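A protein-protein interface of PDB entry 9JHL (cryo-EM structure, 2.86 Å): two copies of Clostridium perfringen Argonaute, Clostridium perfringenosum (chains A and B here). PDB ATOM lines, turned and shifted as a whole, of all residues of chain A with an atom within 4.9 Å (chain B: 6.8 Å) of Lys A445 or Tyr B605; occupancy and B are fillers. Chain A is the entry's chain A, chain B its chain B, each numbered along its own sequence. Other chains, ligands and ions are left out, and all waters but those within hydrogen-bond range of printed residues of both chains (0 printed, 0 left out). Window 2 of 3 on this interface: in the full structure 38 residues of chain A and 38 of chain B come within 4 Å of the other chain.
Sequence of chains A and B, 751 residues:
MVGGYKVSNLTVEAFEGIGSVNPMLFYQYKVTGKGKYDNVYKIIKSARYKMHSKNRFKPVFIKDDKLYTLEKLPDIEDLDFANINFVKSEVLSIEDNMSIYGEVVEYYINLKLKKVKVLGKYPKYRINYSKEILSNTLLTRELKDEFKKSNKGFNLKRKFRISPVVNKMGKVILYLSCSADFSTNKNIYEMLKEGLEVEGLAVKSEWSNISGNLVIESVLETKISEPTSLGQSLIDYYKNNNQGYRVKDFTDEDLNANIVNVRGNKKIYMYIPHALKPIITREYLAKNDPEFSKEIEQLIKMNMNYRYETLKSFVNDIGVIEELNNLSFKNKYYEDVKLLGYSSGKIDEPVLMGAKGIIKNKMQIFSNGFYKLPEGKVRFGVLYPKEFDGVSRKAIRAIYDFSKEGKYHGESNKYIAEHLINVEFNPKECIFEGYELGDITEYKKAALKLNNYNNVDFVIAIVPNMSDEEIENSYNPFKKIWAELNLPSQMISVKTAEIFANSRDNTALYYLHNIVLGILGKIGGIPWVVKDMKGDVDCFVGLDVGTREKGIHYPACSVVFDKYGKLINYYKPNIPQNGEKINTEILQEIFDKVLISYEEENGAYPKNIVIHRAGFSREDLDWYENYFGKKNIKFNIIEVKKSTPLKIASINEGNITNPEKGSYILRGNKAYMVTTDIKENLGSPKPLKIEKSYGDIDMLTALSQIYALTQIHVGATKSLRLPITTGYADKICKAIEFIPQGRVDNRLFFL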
ATOM      1  N   THR A 441      12.758  20.390  -1.001  1.00  0.00           N
ATOM      2  CA  THR A 441      12.817  21.210   0.202  1.00  0.00           C
ATOM      3  C   THR A 441      13.579  20.514   1.322  1.00  0.00           C
ATOM      4  O   THR A 441      14.178  21.186   2.165  1.00  0.00           O
ATOM      5  CB  THR A 441      11.407  21.602   0.655  1.00  0.00           C
ATOM      6  OG1 THR A 441      11.492  22.479   1.784  1.00  0.00           O
ATOM      7  CG2 THR A 441      10.573  20.394   1.016  1.00  0.00           C
ATOM      8  N   GLU A 442      13.638  19.181   1.310  1.00  0.00           N
ATOM      9  CA  GLU A 442      14.455  18.486   2.295  1.00  0.00           C
ATOM     10  C   GLU A 442      15.933  18.607   1.960  1.00  0.00           C
ATOM     11  O   GLU A 442      16.775  18.650   2.861  1.00  0.00           O
ATOM     12  CB  GLU A 442      14.037  17.023   2.392  1.00  0.00           C
ATOM     13  CG  GLU A 442      12.650  16.827   2.972  1.00  0.00           C
ATOM     14  CD  GLU A 442      12.559  17.237   4.429  1.00  0.00           C
ATOM     15  OE1 GLU A 442      13.561  17.095   5.162  1.00  0.00           O
ATOM     16  OE2 GLU A 442      11.478  17.697   4.848  1.00  0.00           O
ATOM     17  N   TYR A 443      16.262  18.695   0.670  1.00  0.00           N
ATOM     18  CA  TYR A 443      17.630  18.992   0.255  1.00  0.00           C
ATOM     19  C   TYR A 443      18.045  20.387   0.693  1.00  0.00           C
ATOM     20  O   TYR A 443      19.154  20.589   1.209  1.00  0.00           O
ATOM     21  CB  TYR A 443      17.739  18.872  -1.259  1.00  0.00           C
ATOM     22  CG  TYR A 443      17.604  17.480  -1.808  1.00  0.00           C
ATOM     23  CD1 TYR A 443      17.862  16.368  -1.024  1.00  0.00           C
ATOM     24  CD2 TYR A 443      17.190  17.281  -3.113  1.00  0.00           C
ATOM     25  CE1 TYR A 443      17.737  15.098  -1.537  1.00  0.00           C
ATOM     26  CE2 TYR A 443      17.059  16.022  -3.630  1.00  0.00           C
ATOM     27  CZ  TYR A 443      17.333  14.935  -2.843  1.00  0.00           C
ATOM     28  OH  TYR A 443      17.196  13.680  -3.375  1.00  0.00           O
ATOM     29  N   LYS A 444      17.157  21.362   0.505  1.00  0.00           N
ATOM     30  CA  LYS A 444      17.459  22.733   0.900  1.00  0.00           C
ATOM     31  C   LYS A 444      17.573  22.860   2.418  1.00  0.00           C
ATOM     32  O   LYS A 444      18.450  23.570   2.926  1.00  0.00           O
ATOM     33  CB  LYS A 444      16.385  23.661   0.345  1.00  0.00           C
ATOM     34  CG  LYS A 444      16.322  23.702  -1.172  1.00  0.00           C
ATOM     35  CD  LYS A 444      15.264  24.674  -1.636  1.00  0.00           C
ATOM     36  CE  LYS A 444      15.093  24.683  -3.145  1.00  0.00           C
ATOM     37  NZ  LYS A 444      16.273  25.261  -3.840  1.00  0.00           N
ATOM     38  N   LYS A 445      16.736  22.133   3.159  1.00  0.00           N
ATOM     39  CA  LYS A 445      16.850  22.145   4.612  1.00  0.00           C
ATOM     40  C   LYS A 445      18.073  21.376   5.095  1.00  0.00           C
ATOM     41  O   LYS A 445      18.627  21.710   6.142  1.00  0.00           O
ATOM     42  CB  LYS A 445      15.582  21.587   5.251  1.00  0.00           C
ATOM     43  CG  LYS A 445      14.391  22.514   5.158  1.00  0.00           C
ATOM     44  CD  LYS A 445      13.237  21.992   5.980  1.00  0.00           C
ATOM     45  CE  LYS A 445      12.603  20.793   5.316  1.00  0.00           C
ATOM     46  NZ  LYS A 445      11.391  20.334   6.045  1.00  0.00           N
ATOM     47  N   ALA A 446      18.524  20.365   4.346  1.00  0.00           N
ATOM     48  CA  ALA A 446      19.759  19.673   4.704  1.00  0.00           C
ATOM     49  C   ALA A 446      20.970  20.576   4.521  1.00  0.00           C
ATOM     50  O   ALA A 446      21.897  20.563   5.341  1.00  0.00           O
ATOM     51  CB  ALA A 446      19.908  18.404   3.868  1.00  0.00           C
ATOM     52  N   ALA A 447      20.968  21.386   3.463  1.00  0.00           N
ATOM     53  CA  ALA A 447      22.058  22.339   3.268  1.00  0.00           C
ATOM     54  C   ALA A 447      22.033  23.448   4.324  1.00  0.00           C
ATOM     55  O   ALA A 447      23.083  23.850   4.845  1.00  0.00           O
ATOM     56  CB  ALA A 447      21.993  22.915   1.858  1.00  0.00           C
ATOM     57  N   LEU A 448      20.842  23.928   4.687  1.00  0.00           N
ATOM     58  CA  LEU A 448      20.750  24.909   5.768  1.00  0.00           C
ATOM     59  C   LEU A 448      21.123  24.300   7.117  1.00  0.00           C
ATOM     60  O   LEU A 448      21.643  24.994   8.000  1.00  0.00           O
ATOM     61  CB  LEU A 448      19.346  25.487   5.809  1.00  0.00           C
ATOM     62  CG  LEU A 448      19.088  26.356   4.591  1.00  0.00           C
ATOM     63  CD1 LEU A 448      17.635  26.563   4.450  1.00  0.00           C
ATOM     64  CD2 LEU A 448      19.794  27.683   4.745  1.00  0.00           C
ATOM     65  N   LYS A 449      20.880  23.002   7.288  1.00  0.00           N
ATOM     66  CA  LYS A 449      21.290  22.315   8.504  1.00  0.00           C
ATOM     67  C   LYS A 449      22.803  22.167   8.558  1.00  0.00           C
ATOM     68  O   LYS A 449      23.399  22.192   9.641  1.00  0.00           O
ATOM     69  CB  LYS A 449      20.601  20.953   8.573  1.00  0.00           C
ATOM     70  CG  LYS A 449      20.849  20.166   9.841  1.00  0.00           C
ATOM     71  CD  LYS A 449      20.037  18.888   9.845  1.00  0.00           C
ATOM     72  CE  LYS A 449      20.383  18.017  11.039  1.00  0.00           C
ATOM     73  NZ  LYS A 449      20.013  18.666  12.325  1.00  0.00           N
ATOM     74  N   ASP B 538      -1.203  32.460   8.003  1.00  0.00           N
ATOM     75  CA  ASP B 538       0.106  32.440   8.635  1.00  0.00           C
ATOM     76  C   ASP B 538       1.144  33.248   7.877  1.00  0.00           C
ATOM     77  O   ASP B 538       1.948  33.940   8.502  1.00  0.00           O
ATOM     78  CB  ASP B 538       0.594  31.003   8.802  1.00  0.00           C
ATOM     79  CG  ASP B 538      -0.183  30.249   9.850  1.00  0.00           C
ATOM     80  OD1 ASP B 538      -0.684  30.889  10.796  1.00  0.00           O
ATOM     81  OD2 ASP B 538      -0.293  29.016   9.735  1.00  0.00           O
ATOM     82  N   ASP B 592       9.718  26.936  -1.709  1.00  0.00           N
ATOM     83  CA  ASP B 592      10.657  26.356  -0.756  1.00  0.00           C
ATOM     84  C   ASP B 592      11.322  27.441   0.072  1.00  0.00           C
ATOM     85  O   ASP B 592      11.482  27.291   1.286  1.00  0.00           O
ATOM     86  CB  ASP B 592      11.715  25.524  -1.473  1.00  0.00           C
ATOM     87  CG  ASP B 592      11.173  24.238  -2.021  1.00  0.00           C
ATOM     88  OD1 ASP B 592      10.146  23.765  -1.503  1.00  0.00           O
ATOM     89  OD2 ASP B 592      11.784  23.692  -2.961  1.00  0.00           O
ATOM     90  N   LEU B 595       8.625  28.581   2.678  1.00  0.00           N
ATOM     91  CA  LEU B 595       8.389  27.693   3.811  1.00  0.00           C
ATOM     92  C   LEU B 595       9.614  27.604   4.701  1.00  0.00           C
ATOM     93  O   LEU B 595       9.486  27.496   5.925  1.00  0.00           O
ATOM     94  CB  LEU B 595       7.997  26.301   3.330  1.00  0.00           C
ATOM     95  CG  LEU B 595       6.774  26.200   2.428  1.00  0.00           C
ATOM     96  CD1 LEU B 595       6.498  24.769   2.109  1.00  0.00           C
ATOM     97  CD2 LEU B 595       5.575  26.882   2.992  1.00  0.00           C
ATOM     98  N   ILE B 596      10.806  27.679   4.105  1.00  0.00           N
ATOM     99  CA  ILE B 596      12.050  27.725   4.864  1.00  0.00           C
ATOM    100  C   ILE B 596      12.124  28.976   5.726  1.00  0.00           C
ATOM    101  O   ILE B 596      12.503  28.910   6.900  1.00  0.00           O
ATOM    102  CB  ILE B 596      13.241  27.613   3.896  1.00  0.00           C
ATOM    103  CG1 ILE B 596      13.490  26.148   3.539  1.00  0.00           C
ATOM    104  CG2 ILE B 596      14.471  28.333   4.411  1.00  0.00           C
ATOM    105  CD1 ILE B 596      14.404  25.981   2.383  1.00  0.00           C
ATOM    106  N   TYR B 598       9.591  30.895   6.796  1.00  0.00           N
ATOM    107  CA  TYR B 598       8.588  30.857   7.855  1.00  0.00           C
ATOM    108  C   TYR B 598       8.966  29.840   8.928  1.00  0.00           C
ATOM    109  O   TYR B 598       8.696  30.057  10.113  1.00  0.00           O
ATOM    110  CB  TYR B 598       7.205  30.540   7.291  1.00  0.00           C
ATOM    111  CG  TYR B 598       6.092  30.794   8.283  1.00  0.00           C
ATOM    112  CD1 TYR B 598       5.572  32.065   8.449  1.00  0.00           C
ATOM    113  CD2 TYR B 598       5.596  29.776   9.088  1.00  0.00           C
ATOM    114  CE1 TYR B 598       4.566  32.307   9.358  1.00  0.00           C
ATOM    115  CE2 TYR B 598       4.594  30.007   9.999  1.00  0.00           C
ATOM    116  CZ  TYR B 598       4.084  31.273  10.131  1.00  0.00           C
ATOM    117  OH  TYR B 598       3.085  31.508  11.043  1.00  0.00           O
ATOM    118  N   GLU B 599       9.605  28.735   8.538  1.00  0.00           N
ATOM    119  CA  GLU B 599      10.039  27.747   9.519  1.00  0.00           C
ATOM    120  C   GLU B 599      11.234  28.255  10.314  1.00  0.00           C
ATOM    121  O   GLU B 599      11.408  27.893  11.483  1.00  0.00           O
ATOM    122  CB  GLU B 599      10.375  26.435   8.812  1.00  0.00           C
ATOM    123  CG  GLU B 599      10.658  25.261   9.728  1.00  0.00           C
ATOM    124  CD  GLU B 599      10.966  23.993   8.963  1.00  0.00           C
ATOM    125  OE1 GLU B 599      11.029  24.051   7.719  1.00  0.00           O
ATOM    126  OE2 GLU B 599      11.137  22.936   9.603  1.00  0.00           O
ATOM    127  N   ASN B 602       9.656  30.933  12.692  1.00  0.00           N
ATOM    128  CA  ASN B 602       8.496  30.508  13.465  1.00  0.00           C
ATOM    129  C   ASN B 602       8.529  29.067  13.957  1.00  0.00           C
ATOM    130  O   ASN B 602       7.714  28.725  14.817  1.00  0.00           O
ATOM    131  CB  ASN B 602       7.219  30.721  12.643  1.00  0.00           C
ATOM    132  CG  ASN B 602       6.912  32.185  12.422  1.00  0.00           C
ATOM    133  OD1 ASN B 602       7.065  32.704  11.319  1.00  0.00           O
ATOM    134  ND2 ASN B 602       6.456  32.858  13.471  1.00  0.00           N
ATOM    135  N   GLY B 603       9.416  28.213  13.456  1.00  0.00           N
ATOM    136  CA  GLY B 603       9.552  26.873  13.986  1.00  0.00           C
ATOM    137  C   GLY B 603       8.763  25.795  13.278  1.00  0.00           C
ATOM    138  O   GLY B 603       8.965  24.611  13.579  1.00  0.00           O
ATOM    139  N   ALA B 604       7.880  26.151  12.348  1.00  0.00           N
ATOM    140  CA  ALA B 604       7.073  25.161  11.651  1.00  0.00           C
ATOM    141  C   ALA B 604       6.644  25.727  10.307  1.00  0.00           C
ATOM    142  O   ALA B 604       6.817  26.916  10.032  1.00  0.00           O
ATOM    143  CB  ALA B 604       5.848  24.752  12.475  1.00  0.00           C
ATOM    144  N   TYR B 605       6.092  24.851   9.471  1.00  0.00           N
ATOM    145  CA  TYR B 605       5.496  25.278   8.216  1.00  0.00           C
ATOM    146  C   TYR B 605       4.239  26.109   8.475  1.00  0.00           C
ATOM    147  O   TYR B 605       3.552  25.914   9.482  1.00  0.00           O
ATOM    148  CB  TYR B 605       5.138  24.070   7.351  1.00  0.00           C
ATOM    149  CG  TYR B 605       6.297  23.433   6.621  1.00  0.00           C
ATOM    150  CD1 TYR B 605       7.497  24.109   6.453  1.00  0.00           C
ATOM    151  CD2 TYR B 605       6.181  22.154   6.091  1.00  0.00           C
ATOM    152  CE1 TYR B 605       8.551  23.529   5.780  1.00  0.00           C
ATOM    153  CE2 TYR B 605       7.230  21.565   5.421  1.00  0.00           C
ATOM    154  CZ  TYR B 605       8.411  22.257   5.269  1.00  0.00           C
ATOM    155  OH  TYR B 605       9.457  21.670   4.599  1.00  0.00           O
ATOM    156  N   PRO B 606       3.919  27.051   7.587  1.00  0.00           N
ATOM    157  CA  PRO B 606       2.668  27.801   7.737  1.00  0.00           C
ATOM    158  C   PRO B 606       1.467  26.942   7.372  1.00  0.00           C
ATOM    159  O   PRO B 606       1.435  26.311   6.316  1.00  0.00           O
ATOM    160  CB  PRO B 606       2.845  28.977   6.771  1.00  0.00           C
ATOM    161  CG  PRO B 606       3.804  28.514   5.783  1.00  0.00           C
ATOM    162  CD  PRO B 606       4.736  27.580   6.483  1.00  0.00           C
ATOM    163  N   LYS B 607       0.482  26.912   8.268  1.00  0.00           N
ATOM    164  CA  LYS B 607      -0.726  26.139   8.007  1.00  0.00           C
ATOM    165  C   LYS B 607      -1.581  26.797   6.935  1.00  0.00           C
ATOM    166  O   LYS B 607      -2.341  26.119   6.238  1.00  0.00           O
ATOM    167  CB  LYS B 607      -1.531  25.969   9.296  1.00  0.00           C
ATOM    168  CG  LYS B 607      -0.818  25.223  10.407  1.00  0.00           C
ATOM    169  CD  LYS B 607      -0.556  23.778  10.032  1.00  0.00           C
ATOM    170  CE  LYS B 607      -1.838  22.971  10.023  1.00  0.00           C
ATOM    171  NZ  LYS B 607      -1.585  21.531   9.750  1.00  0.00           N
ATOM    172  N   ASN B 608      -1.471  28.115   6.788  1.00  0.00           N
ATOM    173  CA  ASN B 608      -2.291  28.886   5.866  1.00  0.00           C
ATOM    174  C   ASN B 608      -1.440  29.918   5.147  1.00  0.00           C
ATOM    175  O   ASN B 608      -0.743  30.707   5.789  1.00  0.00           O
ATOM    176  CB  ASN B 608      -3.431  29.571   6.603  1.00  0.00           C
ATOM    177  CG  ASN B 608      -4.507  28.607   7.035  1.00  0.00           C
ATOM    178  OD1 ASN B 608      -4.970  27.786   6.251  1.00  0.00           O
ATOM    179  ND2 ASN B 608      -4.889  28.677   8.300  1.00  0.00           N
ATOM    180  N   TYR B 627       1.973  20.601  -4.379  1.00  0.00           N
ATOM    181  CA  TYR B 627       3.038  21.091  -3.509  1.00  0.00           C
ATOM    182  C   TYR B 627       2.544  21.345  -2.092  1.00  0.00           C
ATOM    183  O   TYR B 627       3.190  20.937  -1.123  1.00  0.00           O
ATOM    184  CB  TYR B 627       3.633  22.371  -4.093  1.00  0.00           C
ATOM    185  CG  TYR B 627       4.762  22.950  -3.281  1.00  0.00           C
ATOM    186  CD1 TYR B 627       6.038  22.427  -3.370  1.00  0.00           C
ATOM    187  CD2 TYR B 627       4.551  24.015  -2.419  1.00  0.00           C
ATOM    188  CE1 TYR B 627       7.072  22.951  -2.630  1.00  0.00           C
ATOM    189  CE2 TYR B 627       5.577  24.533  -1.667  1.00  0.00           C
ATOM    190  CZ  TYR B 627       6.834  23.998  -1.782  1.00  0.00           C
ATOM    191  OH  TYR B 627       7.866  24.513  -1.042  1.00  0.00           O
ATOM    192  N   LYS B 631       2.443  18.838   1.781  1.00  0.00           N
ATOM    193  CA  LYS B 631       3.019  19.480   2.953  1.00  0.00           C
ATOM    194  C   LYS B 631       1.966  19.919   3.957  1.00  0.00           C
ATOM    195  O   LYS B 631       2.313  20.586   4.938  1.00  0.00           O
ATOM    196  CB  LYS B 631       3.867  20.664   2.506  1.00  0.00           C
ATOM    197  CG  LYS B 631       4.998  20.216   1.627  1.00  0.00           C
ATOM    198  CD  LYS B 631       5.789  21.356   1.086  1.00  0.00           C
ATOM    199  CE  LYS B 631       6.958  20.843   0.285  1.00  0.00           C
ATOM    200  NZ  LYS B 631       6.506  20.115  -0.933  1.00  0.00           N
ATOM    201  N   ASN B 632       0.698  19.552   3.726  1.00  0.00           N
ATOM    202  CA  ASN B 632      -0.442  19.818   4.610  1.00  0.00           C
ATOM    203  C   ASN B 632      -0.604  21.319   4.860  1.00  0.00           C
ATOM    204  O   ASN B 632      -0.639  21.792   5.996  1.00  0.00           O
ATOM    205  CB  ASN B 632      -0.317  19.034   5.924  1.00  0.00           C
ATOM    206  CG  ASN B 632      -1.628  18.942   6.688  1.00  0.00           C
ATOM    207  OD1 ASN B 632      -2.660  19.442   6.241  1.00  0.00           O
ATOM    208  ND2 ASN B 632      -1.589  18.305   7.852  1.00  0.00           N
ATOM    209  N   ILE B 633      -0.674  22.070   3.766  1.00  0.00           N
ATOM    210  CA  ILE B 633      -0.797  23.521   3.808  1.00  0.00           C
ATOM    211  C   ILE B 633      -2.039  23.911   3.026  1.00  0.00           C
ATOM    212  O   ILE B 633      -2.151  23.598   1.835  1.00  0.00           O
ATOM    213  CB  ILE B 633       0.444  24.219   3.231  1.00  0.00           C
ATOM    214  CG1 ILE B 633       1.677  23.896   4.067  1.00  0.00           C
ATOM    215  CG2 ILE B 633       0.232  25.708   3.182  1.00  0.00           C
ATOM    216  CD1 ILE B 633       2.956  24.311   3.420  1.00  0.00           C
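OE2 of Glu A442 lies within salt-bridge range of NZ of Lys A445.
OH of Tyr B627 lies within hydrogen-bond range of OD1 of Asp B592 (2.4 Å).
O of Tyr B627 lies close to NZ of Lys B631.
Hydrophobic or aromatic side chains of chain B that line the printed part of chain A: Ile B596 and Tyr B605.
Of the 9 printed residues of chain A, 4 touch a printed residue of chain B.
Hydrophobic or aromatic side chains of chain A within 4 Å of the printed part of chain B: Leu A448.
Among the printed residues, no Asp or Glu carboxylate lies within 4 Å of a Lys or Arg side-chain nitrogen of the other chain.
Lys A445 touches just these residues of chain B: Glu B599 (3.5 Å) and Tyr B605 (2.8 Å).
Printed residues of chain A within 4 Å of Lys B631: Thr A441 (3.7 Å).
Of the printed residues of chain A, Glu B599 touches Lys A445 (3.5 Å).
Pro B606 touches none of the printed residues of chain A.
Tyr B627 touches none of the printed residues of chain A.
Thr A441 touches Asp B592.
OH of Tyr B605 touches OG1 of Thr A441, at 3.6 Å.
CE of Lys B631 touches CG2 of Thr A441, at 3.7 Å.
OD2 of Asp B592 touches CE of Lys A444, 3.5 Å away.
Lys A444 touches Ile B596 (CB to CD1, 3.7 Å).
Glu B599 touches Lys A445 (OE1 to CD, 3.5 Å).
Leu A448 touches Ile B596.
No position is printed for both chains.
NZ of Lys A445 sits at hydrogen-bond distance from OH of Tyr B605.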
